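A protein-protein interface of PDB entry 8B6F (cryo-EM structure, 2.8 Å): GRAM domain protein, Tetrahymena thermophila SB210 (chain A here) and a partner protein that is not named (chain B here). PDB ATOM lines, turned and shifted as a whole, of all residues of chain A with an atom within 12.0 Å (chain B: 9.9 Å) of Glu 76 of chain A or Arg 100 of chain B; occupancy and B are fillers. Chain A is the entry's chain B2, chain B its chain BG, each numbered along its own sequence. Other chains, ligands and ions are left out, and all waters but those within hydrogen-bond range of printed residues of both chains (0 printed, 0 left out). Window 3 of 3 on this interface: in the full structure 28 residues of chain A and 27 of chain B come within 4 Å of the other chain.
The side-chain carboxylate of Glu 76 of chain A is in salt-bridge range of the guanidinium group of Arg 100 of chain B (3.0 Å).
Among the printed residues, pairs that only touch across the chains: Asp 79 of chain A with Val 99 of chain B (3.1 Å), Tyr 74 of chain A with Ala 103 of chain B (3.5 Å), Phe 81 of chain A with Ala 103 of chain B (3.5 Å) and Phe 81 of chain A with Glu 106 of chain B (3.6 Å).
Asp 75 of chain A touches none of the printed residues of chain B. Glu 76 of chain A touches just one residue of chain B: Arg 100. Of the printed residues of chain B, Asp 79 of chain A touches Val 99 (3.1 Å). Of the printed residues of chain B, Phe 81 of chain A touches Ala 103 and Glu 106. No residue of chain A comes within 4 Å of Asn 97 of chain B. Val 99 of chain B touches just one residue of chain A: Asp 79 (3.1 Å). Arg 100 of chain B touches one residue of chain A. No residue of chain A comes within 4 Å of His 101 of chain B. Of chain A, only Tyr 74 (3.5 Å) and Phe 81 (3.5 Å) come within 4 Å of Ala 103 of chain B. Leu 104 of chain B touches none of the printed residues of chain A. The nearest residue of chain A that does not touch Arg 100 of chain B is Tyr 74 of chain A (5.2 Å).
Among the printed residues, Asp or Glu carboxylates within 4 Å of a Lys or Arg side-chain nitrogen of the other chain: Glu 76 of chain A with Arg 100 of chain B (3.0 Å).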
ATOM      1  N   PRO A  72     -29.104 -28.905   6.393  1.00  0.00           N
ATOM      2  CA  PRO A  72     -28.749 -27.724   5.599  1.00  0.00           C
ATOM      3  C   PRO A  72     -29.658 -27.559   4.394  1.00  0.00           C
ATOM      4  O   PRO A  72     -30.089 -28.535   3.777  1.00  0.00           O
ATOM      5  CB  PRO A  72     -27.305 -28.004   5.172  1.00  0.00           C
ATOM      6  CG  PRO A  72     -27.196 -29.482   5.184  1.00  0.00           C
ATOM      7  CD  PRO A  72     -28.075 -29.955   6.304  1.00  0.00           C
ATOM      8  N   ARG A  73     -29.943 -26.305   4.059  1.00  0.00           N
ATOM      9  CA  ARG A  73     -30.690 -26.011   2.849  1.00  0.00           C
ATOM     10  C   ARG A  73     -29.820 -26.234   1.618  1.00  0.00           C
ATOM     11  O   ARG A  73     -28.589 -26.167   1.669  1.00  0.00           O
ATOM     12  CB  ARG A  73     -31.206 -24.573   2.874  1.00  0.00           C
ATOM     13  CG  ARG A  73     -32.465 -24.413   3.686  1.00  0.00           C
ATOM     14  CD  ARG A  73     -33.659 -24.898   2.890  1.00  0.00           C
ATOM     15  NE  ARG A  73     -34.814 -25.120   3.745  1.00  0.00           N
ATOM     16  CZ  ARG A  73     -35.106 -26.274   4.328  1.00  0.00           C
ATOM     17  NH1 ARG A  73     -34.343 -27.343   4.177  1.00  0.00           N
ATOM     18  NH2 ARG A  73     -36.188 -26.356   5.088  1.00  0.00           N
ATOM     19  N   TYR A  74     -30.481 -26.498   0.495  1.00  0.00           N
ATOM     20  CA  TYR A  74     -29.811 -26.765  -0.771  1.00  0.00           C
ATOM     21  C   TYR A  74     -30.006 -25.563  -1.683  1.00  0.00           C
ATOM     22  O   TYR A  74     -31.131 -25.264  -2.095  1.00  0.00           O
ATOM     23  CB  TYR A  74     -30.350 -28.037  -1.421  1.00  0.00           C
ATOM     24  CG  TYR A  74     -29.765 -28.305  -2.787  1.00  0.00           C
ATOM     25  CD1 TYR A  74     -28.431 -28.662  -2.931  1.00  0.00           C
ATOM     26  CD2 TYR A  74     -30.545 -28.209  -3.930  1.00  0.00           C
ATOM     27  CE1 TYR A  74     -27.887 -28.910  -4.174  1.00  0.00           C
ATOM     28  CE2 TYR A  74     -30.013 -28.454  -5.179  1.00  0.00           C
ATOM     29  CZ  TYR A  74     -28.683 -28.805  -5.296  1.00  0.00           C
ATOM     30  OH  TYR A  74     -28.146 -29.053  -6.537  1.00  0.00           O
ATOM     31  N   ASP A  75     -28.910 -24.879  -1.994  1.00  0.00           N
ATOM     32  CA  ASP A  75     -28.919 -23.803  -2.979  1.00  0.00           C
ATOM     33  C   ASP A  75     -28.794 -24.447  -4.351  1.00  0.00           C
ATOM     34  O   ASP A  75     -27.711 -24.871  -4.757  1.00  0.00           O
ATOM     35  CB  ASP A  75     -27.791 -22.816  -2.712  1.00  0.00           C
ATOM     36  CG  ASP A  75     -27.769 -21.678  -3.706  1.00  0.00           C
ATOM     37  OD1 ASP A  75     -28.715 -21.577  -4.515  1.00  0.00           O
ATOM     38  OD2 ASP A  75     -26.807 -20.882  -3.681  1.00  0.00           O
ATOM     39  N   GLU A  76     -29.911 -24.517  -5.074  1.00  0.00           N
ATOM     40  CA  GLU A  76     -29.930 -25.210  -6.354  1.00  0.00           C
ATOM     41  C   GLU A  76     -29.283 -24.391  -7.461  1.00  0.00           C
ATOM     42  O   GLU A  76     -28.781 -24.964  -8.433  1.00  0.00           O
ATOM     43  CB  GLU A  76     -31.371 -25.561  -6.724  1.00  0.00           C
ATOM     44  CG  GLU A  76     -31.501 -26.430  -7.958  1.00  0.00           C
ATOM     45  CD  GLU A  76     -32.909 -26.954  -8.145  1.00  0.00           C
ATOM     46  OE1 GLU A  76     -33.784 -26.609  -7.324  1.00  0.00           O
ATOM     47  OE2 GLU A  76     -33.143 -27.710  -9.110  1.00  0.00           O
ATOM     48  N   GLU A  77     -29.286 -23.063  -7.340  1.00  0.00           N
ATOM     49  CA  GLU A  77     -28.650 -22.235  -8.359  1.00  0.00           C
ATOM     50  C   GLU A  77     -27.162 -22.541  -8.465  1.00  0.00           C
ATOM     51  O   GLU A  77     -26.626 -22.676  -9.572  1.00  0.00           O
ATOM     52  CB  GLU A  77     -28.869 -20.757  -8.039  1.00  0.00           C
ATOM     53  CG  GLU A  77     -30.331 -20.343  -8.010  1.00  0.00           C
ATOM     54  CD  GLU A  77     -30.516 -18.897  -7.593  1.00  0.00           C
ATOM     55  OE1 GLU A  77     -29.526 -18.271  -7.159  1.00  0.00           O
ATOM     56  OE2 GLU A  77     -31.650 -18.386  -7.702  1.00  0.00           O
ATOM     57  N   ASN A  78     -26.477 -22.656  -7.329  1.00  0.00           N
ATOM     58  CA  ASN A  78     -25.053 -22.958  -7.298  1.00  0.00           C
ATOM     59  C   ASN A  78     -24.761 -24.428  -7.034  1.00  0.00           C
ATOM     60  O   ASN A  78     -23.591 -24.819  -7.017  1.00  0.00           O
ATOM     61  CB  ASN A  78     -24.360 -22.106  -6.231  1.00  0.00           C
ATOM     62  CG  ASN A  78     -24.607 -20.625  -6.420  1.00  0.00           C
ATOM     63  OD1 ASN A  78     -24.782 -20.153  -7.543  1.00  0.00           O
ATOM     64  ND2 ASN A  78     -24.625 -19.883  -5.319  1.00  0.00           N
ATOM     65  N   ASP A  79     -25.791 -25.252  -6.846  1.00  0.00           N
ATOM     66  CA  ASP A  79     -25.615 -26.671  -6.544  1.00  0.00           C
ATOM     67  C   ASP A  79     -24.734 -26.861  -5.310  1.00  0.00           C
ATOM     68  O   ASP A  79     -23.791 -27.655  -5.304  1.00  0.00           O
ATOM     69  CB  ASP A  79     -25.040 -27.416  -7.751  1.00  0.00           C
ATOM     70  CG  ASP A  79     -24.960 -28.913  -7.527  1.00  0.00           C
ATOM     71  OD1 ASP A  79     -26.024 -29.560  -7.441  1.00  0.00           O
ATOM     72  OD2 ASP A  79     -23.833 -29.442  -7.440  1.00  0.00           O
ATOM     73  N   THR A  80     -25.047 -26.113  -4.257  1.00  0.00           N
ATOM     74  CA  THR A  80     -24.305 -26.160  -3.007  1.00  0.00           C
ATOM     75  C   THR A  80     -25.274 -26.398  -1.859  1.00  0.00           C
ATOM     76  O   THR A  80     -26.494 -26.403  -2.034  1.00  0.00           O
ATOM     77  CB  THR A  80     -23.514 -24.865  -2.769  1.00  0.00           C
ATOM     78  OG1 THR A  80     -24.410 -23.747  -2.768  1.00  0.00           O
ATOM     79  CG2 THR A  80     -22.467 -24.671  -3.853  1.00  0.00           C
ATOM     80  N   PHE A  81     -24.712 -26.596  -0.670  1.00  0.00           N
ATOM     81  CA  PHE A  81     -25.480 -26.731   0.560  1.00  0.00           C
ATOM     82  C   PHE A  81     -25.078 -25.623   1.521  1.00  0.00           C
ATOM     83  O   PHE A  81     -23.888 -25.418   1.780  1.00  0.00           O
ATOM     84  CB  PHE A  81     -25.265 -28.103   1.203  1.00  0.00           C
ATOM     85  CG  PHE A  81     -26.026 -29.209   0.531  1.00  0.00           C
ATOM     86  CD1 PHE A  81     -27.357 -29.430   0.834  1.00  0.00           C
ATOM     87  CD2 PHE A  81     -25.411 -30.024  -0.404  1.00  0.00           C
ATOM     88  CE1 PHE A  81     -28.062 -30.445   0.220  1.00  0.00           C
ATOM     89  CE2 PHE A  81     -26.111 -31.040  -1.023  1.00  0.00           C
ATOM     90  CZ  PHE A  81     -27.440 -31.250  -0.711  1.00  0.00           C
ATOM     91  N   VAL A  82     -26.073 -24.914   2.040  1.00  0.00           N
ATOM     92  CA  VAL A  82     -25.859 -23.798   2.957  1.00  0.00           C
ATOM     93  C   VAL A  82     -26.471 -24.186   4.298  1.00  0.00           C
ATOM     94  O   VAL A  82     -27.528 -24.831   4.325  1.00  0.00           O
ATOM     95  CB  VAL A  82     -26.475 -22.505   2.396  1.00  0.00           C
ATOM     96  CG1 VAL A  82     -27.982 -22.651   2.231  1.00  0.00           C
ATOM     97  CG2 VAL A  82     -26.143 -21.317   3.279  1.00  0.00           C
ATOM     98  N   PRO A  83     -25.852 -23.841   5.429  1.00  0.00           N
ATOM     99  CA  PRO A  83     -26.439 -24.219   6.719  1.00  0.00           C
ATOM    100  C   PRO A  83     -27.821 -23.612   6.909  1.00  0.00           C
ATOM    101  O   PRO A  83     -28.115 -22.513   6.435  1.00  0.00           O
ATOM    102  CB  PRO A  83     -25.438 -23.669   7.744  1.00  0.00           C
ATOM    103  CG  PRO A  83     -24.630 -22.661   7.003  1.00  0.00           C
ATOM    104  CD  PRO A  83     -24.559 -23.160   5.601  1.00  0.00           C
ATOM    105  N   GLN A  86     -28.089 -19.943   8.168  1.00  0.00           N
ATOM    106  CA  GLN A  86     -27.970 -18.830   7.236  1.00  0.00           C
ATOM    107  C   GLN A  86     -29.305 -18.554   6.554  1.00  0.00           C
ATOM    108  O   GLN A  86     -30.047 -19.477   6.209  1.00  0.00           O
ATOM    109  CB  GLN A  86     -26.899 -19.127   6.187  1.00  0.00           C
ATOM    110  CG  GLN A  86     -26.746 -18.033   5.138  1.00  0.00           C
ATOM    111  CD  GLN A  86     -25.598 -18.296   4.188  1.00  0.00           C
ATOM    112  OE1 GLN A  86     -24.695 -19.074   4.487  1.00  0.00           O
ATOM    113  NE2 GLN A  86     -25.633 -17.649   3.027  1.00  0.00           N
ATOM    114  N   THR A  88     -31.649 -17.193   3.471  1.00  0.00           N
ATOM    115  CA  THR A  88     -31.622 -17.126   2.017  1.00  0.00           C
ATOM    116  C   THR A  88     -32.980 -16.665   1.511  1.00  0.00           C
ATOM    117  O   THR A  88     -33.995 -16.776   2.202  1.00  0.00           O
ATOM    118  CB  THR A  88     -31.257 -18.478   1.388  1.00  0.00           C
ATOM    119  OG1 THR A  88     -32.199 -19.476   1.803  1.00  0.00           O
ATOM    120  CG2 THR A  88     -29.855 -18.900   1.802  1.00  0.00           C
ATOM    121  N   ALA A  89     -32.984 -16.138   0.284  1.00  0.00           N
ATOM    122  CA  ALA A  89     -34.229 -15.663  -0.312  1.00  0.00           C
ATOM    123  C   ALA A  89     -35.221 -16.805  -0.493  1.00  0.00           C
ATOM    124  O   ALA A  89     -36.427 -16.630  -0.278  1.00  0.00           O
ATOM    125  CB  ALA A  89     -33.944 -14.986  -1.652  1.00  0.00           C
ATOM    126  N   ASP A  90     -34.735 -17.977  -0.889  1.00  0.00           N
ATOM    127  CA  ASP A  90     -35.591 -19.135  -1.110  1.00  0.00           C
ATOM    128  C   ASP A  90     -35.991 -19.833   0.183  1.00  0.00           C
ATOM    129  O   ASP A  90     -36.792 -20.773   0.135  1.00  0.00           O
ATOM    130  CB  ASP A  90     -34.884 -20.136  -2.030  1.00  0.00           C
ATOM    131  CG  ASP A  90     -34.368 -19.494  -3.302  1.00  0.00           C
ATOM    132  OD1 ASP A  90     -34.972 -18.501  -3.759  1.00  0.00           O
ATOM    133  OD2 ASP A  90     -33.356 -19.982  -3.849  1.00  0.00           O
ATOM    134  N   HIS A  91     -35.462 -19.402   1.327  1.00  0.00           N
ATOM    135  CA  HIS A  91     -35.773 -20.058   2.590  1.00  0.00           C
ATOM    136  C   HIS A  91     -37.267 -19.976   2.877  1.00  0.00           C
ATOM    137  O   HIS A  91     -37.919 -18.969   2.591  1.00  0.00           O
ATOM    138  CB  HIS A  91     -34.978 -19.410   3.726  1.00  0.00           C
ATOM    139  CG  HIS A  91     -34.801 -20.295   4.921  1.00  0.00           C
ATOM    140  ND1 HIS A  91     -35.674 -20.289   5.988  1.00  0.00           N
ATOM    141  CD2 HIS A  91     -33.850 -21.210   5.219  1.00  0.00           C
ATOM    142  CE1 HIS A  91     -35.268 -21.165   6.890  1.00  0.00           C
ATOM    143  NE2 HIS A  91     -34.163 -21.737   6.448  1.00  0.00           N
ATOM    144  N   PHE B  92     -28.653 -32.099 -22.155  1.00  0.00           N
ATOM    145  CA  PHE B  92     -28.806 -31.055 -21.147  1.00  0.00           C
ATOM    146  C   PHE B  92     -29.800 -31.469 -20.069  1.00  0.00           C
ATOM    147  O   PHE B  92     -29.540 -31.295 -18.873  1.00  0.00           O
ATOM    148  CB  PHE B  92     -29.239 -29.753 -21.811  1.00  0.00           C
ATOM    149  CG  PHE B  92     -28.322 -29.313 -22.907  1.00  0.00           C
ATOM    150  CD1 PHE B  92     -27.185 -28.590 -22.613  1.00  0.00           C
ATOM    151  CD2 PHE B  92     -28.585 -29.636 -24.225  1.00  0.00           C
ATOM    152  CE1 PHE B  92     -26.333 -28.185 -23.609  1.00  0.00           C
ATOM    153  CE2 PHE B  92     -27.733 -29.233 -25.230  1.00  0.00           C
ATOM    154  CZ  PHE B  92     -26.602 -28.508 -24.920  1.00  0.00           C
ATOM    155  N   MET B  93     -30.943 -32.019 -20.471  1.00  0.00           N
ATOM    156  CA  MET B  93     -31.912 -32.491 -19.489  1.00  0.00           C
ATOM    157  C   MET B  93     -31.333 -33.623 -18.654  1.00  0.00           C
ATOM    158  O   MET B  93     -31.583 -33.708 -17.447  1.00  0.00           O
ATOM    159  CB  MET B  93     -33.197 -32.930 -20.185  1.00  0.00           C
ATOM    160  CG  MET B  93     -33.801 -31.849 -21.058  1.00  0.00           C
ATOM    161  SD  MET B  93     -35.436 -32.284 -21.665  1.00  0.00           S
ATOM    162  CE  MET B  93     -36.404 -32.161 -20.167  1.00  0.00           C
ATOM    163  N   GLN B  94     -30.567 -34.511 -19.285  1.00  0.00           N
ATOM    164  CA  GLN B  94     -29.907 -35.576 -18.542  1.00  0.00           C
ATOM    165  C   GLN B  94     -28.941 -35.006 -17.512  1.00  0.00           C
ATOM    166  O   GLN B  94     -28.874 -35.489 -16.377  1.00  0.00           O
ATOM    167  CB  GLN B  94     -29.176 -36.509 -19.508  1.00  0.00           C
ATOM    168  CG  GLN B  94     -28.619 -37.766 -18.864  1.00  0.00           C
ATOM    169  CD  GLN B  94     -29.709 -38.698 -18.375  1.00  0.00           C
ATOM    170  OE1 GLN B  94     -30.891 -38.466 -18.612  1.00  0.00           O
ATOM    171  NE2 GLN B  94     -29.314 -39.763 -17.689  1.00  0.00           N
ATOM    172  N   SER B  95     -28.180 -33.976 -17.889  1.00  0.00           N
ATOM    173  CA  SER B  95     -27.246 -33.369 -16.947  1.00  0.00           C
ATOM    174  C   SER B  95     -27.981 -32.757 -15.763  1.00  0.00           C
ATOM    175  O   SER B  95     -27.579 -32.934 -14.609  1.00  0.00           O
ATOM    176  CB  SER B  95     -26.404 -32.310 -17.658  1.00  0.00           C
ATOM    177  OG  SER B  95     -25.686 -32.872 -18.743  1.00  0.00           O
ATOM    178  N   MET B  96     -29.066 -32.026 -16.030  1.00  0.00           N
ATOM    179  CA  MET B  96     -29.829 -31.428 -14.940  1.00  0.00           C
ATOM    180  C   MET B  96     -30.393 -32.501 -14.022  1.00  0.00           C
ATOM    181  O   MET B  96     -30.319 -32.385 -12.795  1.00  0.00           O
ATOM    182  CB  MET B  96     -30.956 -30.561 -15.498  1.00  0.00           C
ATOM    183  CG  MET B  96     -30.486 -29.451 -16.415  1.00  0.00           C
ATOM    184  SD  MET B  96     -31.849 -28.591 -17.214  1.00  0.00           S
ATOM    185  CE  MET B  96     -31.000 -27.880 -18.620  1.00  0.00           C
ATOM    186  N   ASN B  97     -30.960 -33.558 -14.604  1.00  0.00           N
ATOM    187  CA  ASN B  97     -31.523 -34.636 -13.801  1.00  0.00           C
ATOM    188  C   ASN B  97     -30.450 -35.310 -12.958  1.00  0.00           C
ATOM    189  O   ASN B  97     -30.676 -35.617 -11.781  1.00  0.00           O
ATOM    190  CB  ASN B  97     -32.207 -35.654 -14.712  1.00  0.00           C
ATOM    191  CG  ASN B  97     -32.833 -36.794 -13.942  1.00  0.00           C
ATOM    192  OD1 ASN B  97     -33.987 -36.717 -13.525  1.00  0.00           O
ATOM    193  ND2 ASN B  97     -32.073 -37.864 -13.752  1.00  0.00           N
ATOM    194  N   ASP B  98     -29.276 -35.553 -13.543  1.00  0.00           N
ATOM    195  CA  ASP B  98     -28.190 -36.171 -12.791  1.00  0.00           C
ATOM    196  C   ASP B  98     -27.734 -35.287 -11.638  1.00  0.00           C
ATOM    197  O   ASP B  98     -27.476 -35.782 -10.535  1.00  0.00           O
ATOM    198  CB  ASP B  98     -27.018 -36.473 -13.723  1.00  0.00           C
ATOM    199  CG  ASP B  98     -27.316 -37.603 -14.686  1.00  0.00           C
ATOM    200  OD1 ASP B  98     -28.460 -38.102 -14.682  1.00  0.00           O
ATOM    201  OD2 ASP B  98     -26.405 -37.997 -15.443  1.00  0.00           O
ATOM    202  N   VAL B  99     -27.633 -33.977 -11.866  1.00  0.00           N
ATOM    203  CA  VAL B  99     -27.200 -33.080 -10.798  1.00  0.00           C
ATOM    204  C   VAL B  99     -28.200 -33.094  -9.651  1.00  0.00           C
ATOM    205  O   VAL B  99     -27.817 -33.157  -8.476  1.00  0.00           O
ATOM    206  CB  VAL B  99     -26.980 -31.659 -11.348  1.00  0.00           C
ATOM    207  CG1 VAL B  99     -26.847 -30.659 -10.215  1.00  0.00           C
ATOM    208  CG2 VAL B  99     -25.750 -31.623 -12.232  1.00  0.00           C
ATOM    209  N   ARG B 100     -29.495 -33.025  -9.965  1.00  0.00           N
ATOM    210  CA  ARG B 100     -30.502 -33.067  -8.912  1.00  0.00           C
ATOM    211  C   ARG B 100     -30.454 -34.394  -8.170  1.00  0.00           C
ATOM    212  O   ARG B 100     -30.541 -34.434  -6.939  1.00  0.00           O
ATOM    213  CB  ARG B 100     -31.891 -32.832  -9.501  1.00  0.00           C
ATOM    214  CG  ARG B 100     -32.089 -31.450 -10.097  1.00  0.00           C
ATOM    215  CD  ARG B 100     -33.541 -31.238 -10.477  1.00  0.00           C
ATOM    216  NE  ARG B 100     -33.799 -29.896 -10.988  1.00  0.00           N
ATOM    217  CZ  ARG B 100     -33.793 -29.561 -12.271  1.00  0.00           C
ATOM    218  NH1 ARG B 100     -33.531 -30.446 -13.218  1.00  0.00           N
ATOM    219  NH2 ARG B 100     -34.071 -28.308 -12.615  1.00  0.00           N
ATOM    220  N   HIS B 101     -30.314 -35.495  -8.910  1.00  0.00           N
ATOM    221  CA  HIS B 101     -30.247 -36.812  -8.288  1.00  0.00           C
ATOM    222  C   HIS B 101     -29.056 -36.912  -7.346  1.00  0.00           C
ATOM    223  O   HIS B 101     -29.171 -37.448  -6.239  1.00  0.00           O
ATOM    224  CB  HIS B 101     -30.171 -37.883  -9.375  1.00  0.00           C
ATOM    225  CG  HIS B 101     -30.224 -39.284  -8.855  1.00  0.00           C
ATOM    226  ND1 HIS B 101     -29.099 -40.065  -8.709  1.00  0.00           N
ATOM    227  CD2 HIS B 101     -31.267 -40.048  -8.455  1.00  0.00           C
ATOM    228  CE1 HIS B 101     -29.445 -41.248  -8.237  1.00  0.00           C
ATOM    229  NE2 HIS B 101     -30.755 -41.266  -8.076  1.00  0.00           N
ATOM    230  N   LEU B 102     -27.899 -36.400  -7.770  1.00  0.00           N
ATOM    231  CA  LEU B 102     -26.707 -36.444  -6.930  1.00  0.00           C
ATOM    232  C   LEU B 102     -26.831 -35.529  -5.719  1.00  0.00           C
ATOM    233  O   LEU B 102     -26.295 -35.846  -4.650  1.00  0.00           O
ATOM    234  CB  LEU B 102     -25.475 -36.076  -7.754  1.00  0.00           C
ATOM    235  CG  LEU B 102     -25.125 -37.063  -8.869  1.00  0.00           C
ATOM    236  CD1 LEU B 102     -24.003 -36.518  -9.729  1.00  0.00           C
ATOM    237  CD2 LEU B 102     -24.742 -38.420  -8.296  1.00  0.00           C
ATOM    238  N   ALA B 103     -27.522 -34.397  -5.857  1.00  0.00           N
ATOM    239  CA  ALA B 103     -27.759 -33.539  -4.701  1.00  0.00           C
ATOM    240  C   ALA B 103     -28.593 -34.260  -3.651  1.00  0.00           C
ATOM    241  O   ALA B 103     -28.290 -34.204  -2.455  1.00  0.00           O
ATOM    242  CB  ALA B 103     -28.444 -32.245  -5.138  1.00  0.00           C
ATOM    243  N   LEU B 104     -29.665 -34.932  -4.079  1.00  0.00           N
ATOM    244  CA  LEU B 104     -30.470 -35.692  -3.129  1.00  0.00           C
ATOM    245  C   LEU B 104     -29.657 -36.816  -2.503  1.00  0.00           C
ATOM    246  O   LEU B 104     -29.774 -37.085  -1.301  1.00  0.00           O
ATOM    247  CB  LEU B 104     -31.717 -36.248  -3.816  1.00  0.00           C
ATOM    248  CG  LEU B 104     -32.933 -35.323  -3.741  1.00  0.00           C
ATOM    249  CD1 LEU B 104     -32.703 -34.080  -4.574  1.00  0.00           C
ATOM    250  CD2 LEU B 104     -34.199 -36.031  -4.183  1.00  0.00           C
ATOM    251  N   ARG B 105     -28.831 -37.493  -3.305  1.00  0.00           N
ATOM    252  CA  ARG B 105     -27.985 -38.556  -2.772  1.00  0.00           C
ATOM    253  C   ARG B 105     -26.996 -38.018  -1.746  1.00  0.00           C
ATOM    254  O   ARG B 105     -26.749 -38.658  -0.719  1.00  0.00           O
ATOM    255  CB  ARG B 105     -27.245 -39.262  -3.907  1.00  0.00           C
ATOM    256  CG  ARG B 105     -28.070 -40.339  -4.591  1.00  0.00           C
ATOM    257  CD  ARG B 105     -27.309 -41.009  -5.724  1.00  0.00           C
ATOM    258  NE  ARG B 105     -26.044 -41.583  -5.282  1.00  0.00           N
ATOM    259  CZ  ARG B 105     -25.220 -42.267  -6.064  1.00  0.00           C
ATOM    260  NH1 ARG B 105     -25.498 -42.488  -7.337  1.00  0.00           N
ATOM    261  NH2 ARG B 105     -24.088 -42.743  -5.552  1.00  0.00           N
ATOM    262  N   GLU B 106     -26.419 -36.842  -2.005  1.00  0.00           N
ATOM    263  CA  GLU B 106     -25.500 -36.249  -1.039  1.00  0.00           C
ATOM    264  C   GLU B 106     -26.209 -35.919   0.267  1.00  0.00           C
ATOM    265  O   GLU B 106     -25.674 -36.171   1.351  1.00  0.00           O
ATOM    266  CB  GLU B 106     -24.854 -34.994  -1.623  1.00  0.00           C
ATOM    267  CG  GLU B 106     -23.786 -35.282  -2.664  1.00  0.00           C
ATOM    268  CD  GLU B 106     -23.115 -34.023  -3.169  1.00  0.00           C
ATOM    269  OE1 GLU B 106     -23.602 -32.920  -2.842  1.00  0.00           O
ATOM    270  OE2 GLU B 106     -22.097 -34.132  -3.884  1.00  0.00           O
ATOM    271  N   ARG B 107     -27.414 -35.354   0.187  1.00  0.00           N
ATOM    272  CA  ARG B 107     -28.169 -35.074   1.401  1.00  0.00           C
ATOM    273  C   ARG B 107     -28.425 -36.357   2.181  1.00  0.00           C
ATOM    274  O   ARG B 107     -28.240 -36.404   3.403  1.00  0.00           O
ATOM    275  CB  ARG B 107     -29.486 -34.381   1.054  1.00  0.00           C
ATOM    276  CG  ARG B 107     -30.323 -34.008   2.269  1.00  0.00           C
ATOM    277  CD  ARG B 107     -31.704 -33.526   1.871  1.00  0.00           C
ATOM    278  NE  ARG B 107     -32.455 -34.554   1.157  1.00  0.00           N
ATOM    279  CZ  ARG B 107     -33.118 -35.542   1.739  1.00  0.00           C
ATOM    280  NH1 ARG B 107     -33.143 -35.678   3.054  1.00  0.00           N
ATOM    281  NH2 ARG B 107     -33.774 -36.416   0.983  1.00  0.00           N
ATOM    282  N   ASN B 108     -28.853 -37.413   1.487  1.00  0.00           N
ATOM    283  CA  ASN B 108     -29.133 -38.676   2.162  1.00  0.00           C
ATOM    284  C   ASN B 108     -27.868 -39.268   2.766  1.00  0.00           C
ATOM    285  O   ASN B 108     -27.899 -39.828   3.867  1.00  0.00           O
ATOM    286  CB  ASN B 108     -29.775 -39.665   1.189  1.00  0.00           C
ATOM    287  CG  ASN B 108     -31.250 -39.401   0.981  1.00  0.00           C
ATOM    288  OD1 ASN B 108     -31.943 -38.938   1.884  1.00  0.00           O
ATOM    289  ND2 ASN B 108     -31.740 -39.698  -0.215  1.00  0.00           N
